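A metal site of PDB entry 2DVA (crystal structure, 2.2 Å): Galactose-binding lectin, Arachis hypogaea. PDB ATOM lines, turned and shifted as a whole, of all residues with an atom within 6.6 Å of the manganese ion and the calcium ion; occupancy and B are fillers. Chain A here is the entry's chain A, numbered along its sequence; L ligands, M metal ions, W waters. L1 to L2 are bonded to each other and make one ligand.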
ATOM      1  N   ASP A  83      -3.647  26.875  13.582  1.00  0.00           N
ATOM      2  CA  ASP A  83      -4.992  26.412  13.954  1.00  0.00           C
ATOM      3  C   ASP A  83      -6.019  26.454  12.822  1.00  0.00           C
ATOM      4  O   ASP A  83      -7.055  25.785  12.898  1.00  0.00           O
ATOM      5  CB  ASP A  83      -5.508  27.237  15.135  1.00  0.00           C
ATOM      6  CG  ASP A  83      -5.034  26.710  16.461  1.00  0.00           C
ATOM      7  OD1 ASP A  83      -5.720  25.832  17.020  1.00  0.00           O
ATOM      8  OD2 ASP A  83      -3.970  27.154  16.928  1.00  0.00           O
ATOM      9  N   GLY A 103      -4.531  30.614  18.922  1.00  0.00           N
ATOM     10  CA  GLY A 103      -4.946  29.227  18.946  1.00  0.00           C
ATOM     11  C   GLY A 103      -6.326  28.980  18.346  1.00  0.00           C
ATOM     12  O   GLY A 103      -6.646  29.460  17.248  1.00  0.00           O
ATOM     13  N   GLY A 104      -7.150  28.246  19.089  1.00  0.00           N
ATOM     14  CA  GLY A 104      -8.485  27.918  18.626  1.00  0.00           C
ATOM     15  C   GLY A 104      -9.447  29.082  18.458  1.00  0.00           C
ATOM     16  O   GLY A 104     -10.525  28.906  17.883  1.00  0.00           O
ATOM     17  N   THR A 105      -9.071  30.263  18.949  1.00  0.00           N
ATOM     18  CA  THR A 105      -9.904  31.452  18.830  1.00  0.00           C
ATOM     19  C   THR A 105      -9.873  31.978  17.398  1.00  0.00           C
ATOM     20  O   THR A 105     -10.654  32.858  17.033  1.00  0.00           O
ATOM     21  CB  THR A 105      -9.430  32.583  19.756  1.00  0.00           C
ATOM     22  OG1 THR A 105      -8.156  33.055  19.314  1.00  0.00           O
ATOM     23  CG2 THR A 105      -9.299  32.089  21.191  1.00  0.00           C
ATOM     24  N   LEU A 106      -8.942  31.454  16.601  1.00  0.00           N
ATOM     25  CA  LEU A 106      -8.768  31.856  15.209  1.00  0.00           C
ATOM     26  C   LEU A 106      -8.582  33.347  15.036  1.00  0.00           C
ATOM     27  O   LEU A 106      -8.748  33.883  13.926  1.00  0.00           O
ATOM     28  CB  LEU A 106      -9.951  31.361  14.365  1.00  0.00           C
ATOM     29  CG  LEU A 106     -10.157  29.850  14.336  1.00  0.00           C
ATOM     30  CD1 LEU A 106     -11.362  29.522  13.452  1.00  0.00           C
ATOM     31  CD2 LEU A 106      -8.902  29.160  13.815  1.00  0.00           C
ATOM     32  N   GLU A 121     -15.118  29.067   8.842  1.00  0.00           N
ATOM     33  CA  GLU A 121     -13.811  28.607   9.286  1.00  0.00           C
ATOM     34  C   GLU A 121     -13.349  27.327   8.619  1.00  0.00           C
ATOM     35  O   GLU A 121     -14.159  26.498   8.187  1.00  0.00           O
ATOM     36  CB  GLU A 121     -13.795  28.434  10.811  1.00  0.00           C
ATOM     37  CG  GLU A 121     -14.832  27.437  11.297  1.00  0.00           C
ATOM     38  CD  GLU A 121     -14.565  26.970  12.710  1.00  0.00           C
ATOM     39  OE1 GLU A 121     -14.648  27.794  13.643  1.00  0.00           O
ATOM     40  OE2 GLU A 121     -14.270  25.776  12.875  1.00  0.00           O
ATOM     41  N   ASP A 123     -10.989  24.886   9.991  1.00  0.00           N
ATOM     42  CA  ASP A 123     -10.353  24.435  11.207  1.00  0.00           C
ATOM     43  C   ASP A 123      -9.490  23.190  11.107  1.00  0.00           C
ATOM     44  O   ASP A 123      -9.980  22.139  10.693  1.00  0.00           O
ATOM     45  CB  ASP A 123     -11.461  24.192  12.227  1.00  0.00           C
ATOM     46  CG  ASP A 123     -11.013  24.448  13.609  1.00  0.00           C
ATOM     47  OD1 ASP A 123      -9.814  24.228  13.885  1.00  0.00           O
ATOM     48  OD2 ASP A 123     -11.860  24.845  14.432  1.00  0.00           O
ATOM     49  N   THR A 124      -8.227  23.283  11.527  1.00  0.00           N
ATOM     50  CA  THR A 124      -7.315  22.139  11.450  1.00  0.00           C
ATOM     51  C   THR A 124      -6.869  21.552  12.792  1.00  0.00           C
ATOM     52  O   THR A 124      -5.887  20.802  12.847  1.00  0.00           O
ATOM     53  CB  THR A 124      -6.036  22.481  10.670  1.00  0.00           C
ATOM     54  OG1 THR A 124      -5.244  23.398  11.437  1.00  0.00           O
ATOM     55  CG2 THR A 124      -6.391  23.120   9.331  1.00  0.00           C
ATOM     56  N   TYR A 125      -7.563  21.888  13.877  1.00  0.00           N
ATOM     57  CA  TYR A 125      -7.220  21.359  15.190  1.00  0.00           C
ATOM     58  C   TYR A 125      -8.484  21.237  16.020  1.00  0.00           C
ATOM     59  O   TYR A 125      -9.303  22.145  16.043  1.00  0.00           O
ATOM     60  CB  TYR A 125      -6.199  22.240  15.908  1.00  0.00           C
ATOM     61  CG  TYR A 125      -5.878  21.742  17.297  1.00  0.00           C
ATOM     62  CD1 TYR A 125      -6.658  22.130  18.389  1.00  0.00           C
ATOM     63  CD2 TYR A 125      -4.850  20.824  17.515  1.00  0.00           C
ATOM     64  CE1 TYR A 125      -6.438  21.606  19.654  1.00  0.00           C
ATOM     65  CE2 TYR A 125      -4.617  20.283  18.787  1.00  0.00           C
ATOM     66  CZ  TYR A 125      -5.415  20.676  19.857  1.00  0.00           C
ATOM     67  OH  TYR A 125      -5.215  20.157  21.113  1.00  0.00           O
ATOM     68  N   SER A 126      -8.656  20.122  16.717  1.00  0.00           N
ATOM     69  CA  SER A 126      -9.868  19.929  17.514  1.00  0.00           C
ATOM     70  C   SER A 126      -9.825  20.489  18.943  1.00  0.00           C
ATOM     71  O   SER A 126      -9.318  19.828  19.855  1.00  0.00           O
ATOM     72  CB  SER A 126     -10.215  18.447  17.571  1.00  0.00           C
ATOM     73  OG  SER A 126     -11.494  18.249  18.135  1.00  0.00           O
ATOM     74  N   ASN A 127     -10.353  21.695  19.125  1.00  0.00           N
ATOM     75  CA  ASN A 127     -10.410  22.327  20.445  1.00  0.00           C
ATOM     76  C   ASN A 127     -11.704  21.911  21.129  1.00  0.00           C
ATOM     77  O   ASN A 127     -12.783  22.411  20.816  1.00  0.00           O
ATOM     78  CB  ASN A 127     -10.386  23.852  20.350  1.00  0.00           C
ATOM     79  CG  ASN A 127      -9.083  24.375  19.792  1.00  0.00           C
ATOM     80  OD1 ASN A 127      -8.821  24.223  18.605  1.00  0.00           O
ATOM     81  ND2 ASN A 127      -8.260  24.992  20.631  1.00  0.00           N
ATOM     82  N   TYR A 130     -14.158  24.321  22.562  1.00  0.00           N
ATOM     83  CA  TYR A 130     -15.048  25.027  21.633  1.00  0.00           C
ATOM     84  C   TYR A 130     -15.969  24.024  20.943  1.00  0.00           C
ATOM     85  O   TYR A 130     -16.616  24.354  19.943  1.00  0.00           O
ATOM     86  CB  TYR A 130     -14.242  25.808  20.599  1.00  0.00           C
ATOM     87  CG  TYR A 130     -13.301  26.814  21.213  1.00  0.00           C
ATOM     88  CD1 TYR A 130     -13.728  27.648  22.247  1.00  0.00           C
ATOM     89  CD2 TYR A 130     -11.984  26.936  20.758  1.00  0.00           C
ATOM     90  CE1 TYR A 130     -12.857  28.575  22.830  1.00  0.00           C
ATOM     91  CE2 TYR A 130     -11.111  27.863  21.327  1.00  0.00           C
ATOM     92  CZ  TYR A 130     -11.550  28.680  22.367  1.00  0.00           C
ATOM     93  OH  TYR A 130     -10.685  29.577  22.948  1.00  0.00           O
ATOM     94  N   ASN A 131     -16.009  22.817  21.487  1.00  0.00           N
ATOM     95  CA  ASN A 131     -16.844  21.747  20.960  1.00  0.00           C
ATOM     96  C   ASN A 131     -16.571  21.369  19.505  1.00  0.00           C
ATOM     97  O   ASN A 131     -17.486  20.999  18.777  1.00  0.00           O
ATOM     98  CB  ASN A 131     -18.325  22.101  21.128  1.00  0.00           C
ATOM     99  CG  ASN A 131     -18.746  22.185  22.589  1.00  0.00           C
ATOM    100  OD1 ASN A 131     -18.619  21.215  23.334  1.00  0.00           O
ATOM    101  ND2 ASN A 131     -19.241  23.342  23.007  1.00  0.00           N
ATOM    102  N   ASP A 132     -15.307  21.447  19.078  1.00  0.00           N
ATOM    103  CA  ASP A 132     -14.953  21.079  17.717  1.00  0.00           C
ATOM    104  C   ASP A 132     -15.203  19.612  17.407  1.00  0.00           C
ATOM    105  O   ASP A 132     -15.130  18.763  18.292  1.00  0.00           O
ATOM    106  CB  ASP A 132     -13.475  21.312  17.430  1.00  0.00           C
ATOM    107  CG  ASP A 132     -13.143  22.739  17.157  1.00  0.00           C
ATOM    108  OD1 ASP A 132     -13.966  23.442  16.534  1.00  0.00           O
ATOM    109  OD2 ASP A 132     -12.051  23.163  17.562  1.00  0.00           O
ATOM    110  N   PRO A 133     -15.503  19.304  16.138  1.00  0.00           N
ATOM    111  CA  PRO A 133     -15.733  17.898  15.761  1.00  0.00           C
ATOM    112  C   PRO A 133     -14.363  17.262  15.971  1.00  0.00           C
ATOM    113  O   PRO A 133     -13.385  17.955  16.203  1.00  0.00           O
ATOM    114  CB  PRO A 133     -16.098  17.990  14.277  1.00  0.00           C
ATOM    115  CG  PRO A 133     -16.677  19.357  14.146  1.00  0.00           C
ATOM    116  CD  PRO A 133     -15.776  20.198  15.007  1.00  0.00           C
ATOM    117  N   HIS A 137     -12.324  20.428   9.734  1.00  0.00           N
ATOM    118  CA  HIS A 137     -13.674  20.745   9.325  1.00  0.00           C
ATOM    119  C   HIS A 137     -13.875  22.184   8.856  1.00  0.00           C
ATOM    120  O   HIS A 137     -13.054  23.063   9.113  1.00  0.00           O
ATOM    121  CB  HIS A 137     -14.621  20.497  10.495  1.00  0.00           C
ATOM    122  CG  HIS A 137     -14.221  21.228  11.744  1.00  0.00           C
ATOM    123  ND1 HIS A 137     -13.181  20.823  12.554  1.00  0.00           N
ATOM    124  CD2 HIS A 137     -14.695  22.377  12.292  1.00  0.00           C
ATOM    125  CE1 HIS A 137     -13.033  21.684  13.539  1.00  0.00           C
ATOM    126  NE2 HIS A 137     -13.932  22.631  13.406  1.00  0.00           N
ATOM    127  N   GLY A 139     -16.624  25.204   9.147  1.00  0.00           N
ATOM    128  CA  GLY A 139     -17.746  25.542   9.991  1.00  0.00           C
ATOM    129  C   GLY A 139     -18.299  26.931   9.713  1.00  0.00           C
ATOM    130  O   GLY A 139     -17.602  27.792   9.175  1.00  0.00           O
ATOM    131  N   ASP A 141     -19.681  30.077  11.559  1.00  0.00           N
ATOM    132  CA  ASP A 141     -19.692  30.670  12.891  1.00  0.00           C
ATOM    133  C   ASP A 141     -20.524  31.946  12.994  1.00  0.00           C
ATOM    134  O   ASP A 141     -20.535  32.776  12.086  1.00  0.00           O
ATOM    135  CB  ASP A 141     -18.255  30.988  13.334  1.00  0.00           C
ATOM    136  CG  ASP A 141     -17.349  29.767  13.318  1.00  0.00           C
ATOM    137  OD1 ASP A 141     -17.863  28.625  13.233  1.00  0.00           O
ATOM    138  OD2 ASP A 141     -16.116  29.958  13.411  1.00  0.00           O
ATOM    139  N   VAL A 145     -16.631  30.704  18.031  1.00  0.00           N
ATOM    140  CA  VAL A 145     -15.856  29.675  17.338  1.00  0.00           C
ATOM    141  C   VAL A 145     -16.448  28.306  17.630  1.00  0.00           C
ATOM    142  O   VAL A 145     -15.955  27.290  17.145  1.00  0.00           O
ATOM    143  CB  VAL A 145     -14.353  29.692  17.709  1.00  0.00           C
ATOM    144  CG1 VAL A 145     -13.684  30.917  17.101  1.00  0.00           C
ATOM    145  CG2 VAL A 145     -14.172  29.669  19.212  1.00  0.00           C
ATOM    146  N   ASP A 146     -17.507  28.285  18.434  1.00  0.00           N
ATOM    147  CA  ASP A 146     -18.226  27.052  18.724  1.00  0.00           C
ATOM    148  C   ASP A 146     -19.250  27.100  17.600  1.00  0.00           C
ATOM    149  O   ASP A 146     -20.350  27.647  17.748  1.00  0.00           O
ATOM    150  CB  ASP A 146     -18.941  27.143  20.085  1.00  0.00           C
ATOM    151  CG  ASP A 146     -19.640  25.841  20.460  1.00  0.00           C
ATOM    152  OD1 ASP A 146     -20.087  25.116  19.541  1.00  0.00           O
ATOM    153  OD2 ASP A 146     -19.765  25.533  21.669  1.00  0.00           O
ATOM    154  N   SER A 147     -18.862  26.549  16.457  1.00  0.00           N
ATOM    155  CA  SER A 147     -19.677  26.560  15.252  1.00  0.00           C
ATOM    156  C   SER A 147     -21.159  26.204  15.357  1.00  0.00           C
ATOM    157  O   SER A 147     -21.552  25.243  16.036  1.00  0.00           O
ATOM    158  CB  SER A 147     -19.018  25.660  14.190  1.00  0.00           C
ATOM    159  OG  SER A 147     -17.741  26.166  13.827  1.00  0.00           O
ATOM    160  N   THR A 150     -20.968  22.402  11.383  1.00  0.00           N
ATOM    161  CA  THR A 150     -19.691  22.022  10.774  1.00  0.00           C
ATOM    162  C   THR A 150     -19.864  20.841   9.819  1.00  0.00           C
ATOM    163  O   THR A 150     -20.889  20.163   9.832  1.00  0.00           O
ATOM    164  CB  THR A 150     -18.647  21.600  11.833  1.00  0.00           C
ATOM    165  OG1 THR A 150     -18.946  20.292  12.319  1.00  0.00           O
ATOM    166  CG2 THR A 150     -18.642  22.575  12.985  1.00  0.00           C
HETATM  167  O1  LIG L   1       3.247  23.000  24.862  1.00  0.00           O
HETATM  168  C1  LIG L   1       2.347  23.274  23.806  1.00  0.00           C
HETATM  169  C2  LIG L   1       0.967  23.684  24.314  1.00  0.00           C
HETATM  170  O2  LIG L   1       1.047  24.853  25.301  1.00  0.00           O
HETATM  171  C3  LIG L   1      -0.231  25.295  25.955  1.00  0.00           C
HETATM  172  O3  LIG L   1      -0.773  24.179  26.707  1.00  0.00           O
HETATM  173  C4  LIG L   1      -0.154  23.741  28.078  1.00  0.00           C
HETATM  174  C5  LIG L   1      -1.186  25.758  24.842  1.00  0.00           C
HETATM  175  N1  LIG L   1      -2.351  26.143  25.562  1.00  0.00           N
HETATM  176  C6  LIG L   1      -3.147  27.216  25.266  1.00  0.00           C
HETATM  177  O4  LIG L   1      -2.748  28.233  24.660  1.00  0.00           O
HETATM  178  C7  LIG L   1      -4.594  27.149  25.717  1.00  0.00           C
HETATM  179  C8  LIG L   1      -1.382  24.624  23.809  1.00  0.00           C
HETATM  180  O5  LIG L   1      -2.176  25.153  22.807  1.00  0.00           O
HETATM  181  C9  LIG L   1      -0.038  24.117  23.139  1.00  0.00           C
HETATM  182  O6  LIG L   1       0.486  25.215  22.342  1.00  0.00           O
HETATM  183  C1  LG2 L   2      -3.144  24.532  21.988  1.00  0.00           C
HETATM  184  C2  LG2 L   2      -4.191  25.446  21.384  1.00  0.00           C
HETATM  185  C3  LG2 L   2      -4.880  24.806  20.167  1.00  0.00           C
HETATM  186  C4  LG2 L   2      -3.803  24.321  19.044  1.00  0.00           C
HETATM  187  C5  LG2 L   2      -2.860  23.288  19.726  1.00  0.00           C
HETATM  188  C6  LG2 L   2      -1.740  22.452  19.159  1.00  0.00           C
HETATM  189  O1  LG2 L   2      -5.093  25.729  22.447  1.00  0.00           O
HETATM  190  O2  LG2 L   2      -5.754  25.771  19.575  1.00  0.00           O
HETATM  191  O3  LG2 L   2      -2.957  25.397  18.613  1.00  0.00           O
HETATM  192  O4  LG2 L   2      -2.218  23.984  20.920  1.00  0.00           O
HETATM  193  O5  LG2 L   2      -1.065  21.271  19.533  1.00  0.00           O
HETATM  194 MN    MN M   1     -13.987  24.629  14.697  1.00  0.00          MN
HETATM  195 CA    CA M   2     -10.143  24.490  16.441  1.00  0.00          CA
HETATM  196  O   HOH W   1      -8.000  25.550  15.470  1.00  0.00           O
HETATM  197  O   HOH W   2     -13.805  26.646  15.826  1.00  0.00           O
HETATM  198  O   HOH W   3     -11.400  26.779  16.887  1.00  0.00           O
HETATM  199  O   HOH W   4     -16.255  24.228  14.843  1.00  0.00           O
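The side-chain amide nitrogen (ND2) of Asn 127 is in hydrogen-bond range of an oxygen (O2) of LG2 L2 (2.8 Å).
The backbone NH (N) of Gly 104 lies within hydrogen-bond range of an oxygen (O2) of LG2 L2, at 2.9 Å.
The side-chain carboxylate of Asp 83 sits at hydrogen-bond distance from an oxygen (O2) of LG2 L2, at 2.6 Å.
The nearest printed residue that does not touch the manganese ion is Val 145 (4.1 Å).
The calcium ion is bound by O of Tyr 125 (2.5 Å), OD1 of Asn 127 (2.5 Å), OD2 of Asp 132 (2.6 Å), water W1 (2.6 Å), OD1 of Asp 123 (2.6 Å), water W3 (2.6 Å) and OD2 of Asp 123 (2.7 Å).
The calcium ion has seven donor atoms within binding distance.
Water W2 lies within hydrogen-bond range of O of Val 145 (2.6 Å) and OE1 of Glu 121 (2.6 Å).
The manganese ion is bound by OD2 of Asp 123, OE2 of Glu 121, OD1 of Asp 132, water W4, water W2 and NE2 of His 137.
The manganese ion has six donor atoms within binding distance.
Four residues have an atom within 4 Å of the calcium ion: Asp 123, Tyr 125, Asn 127 and Asp 132.
OE1 of Glu 121 sits close to OD2 of Asp 141 (2.6 Å).
N of Glu 121 sits at hydrogen-bond distance from O of Gly 139 (2.8 Å).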
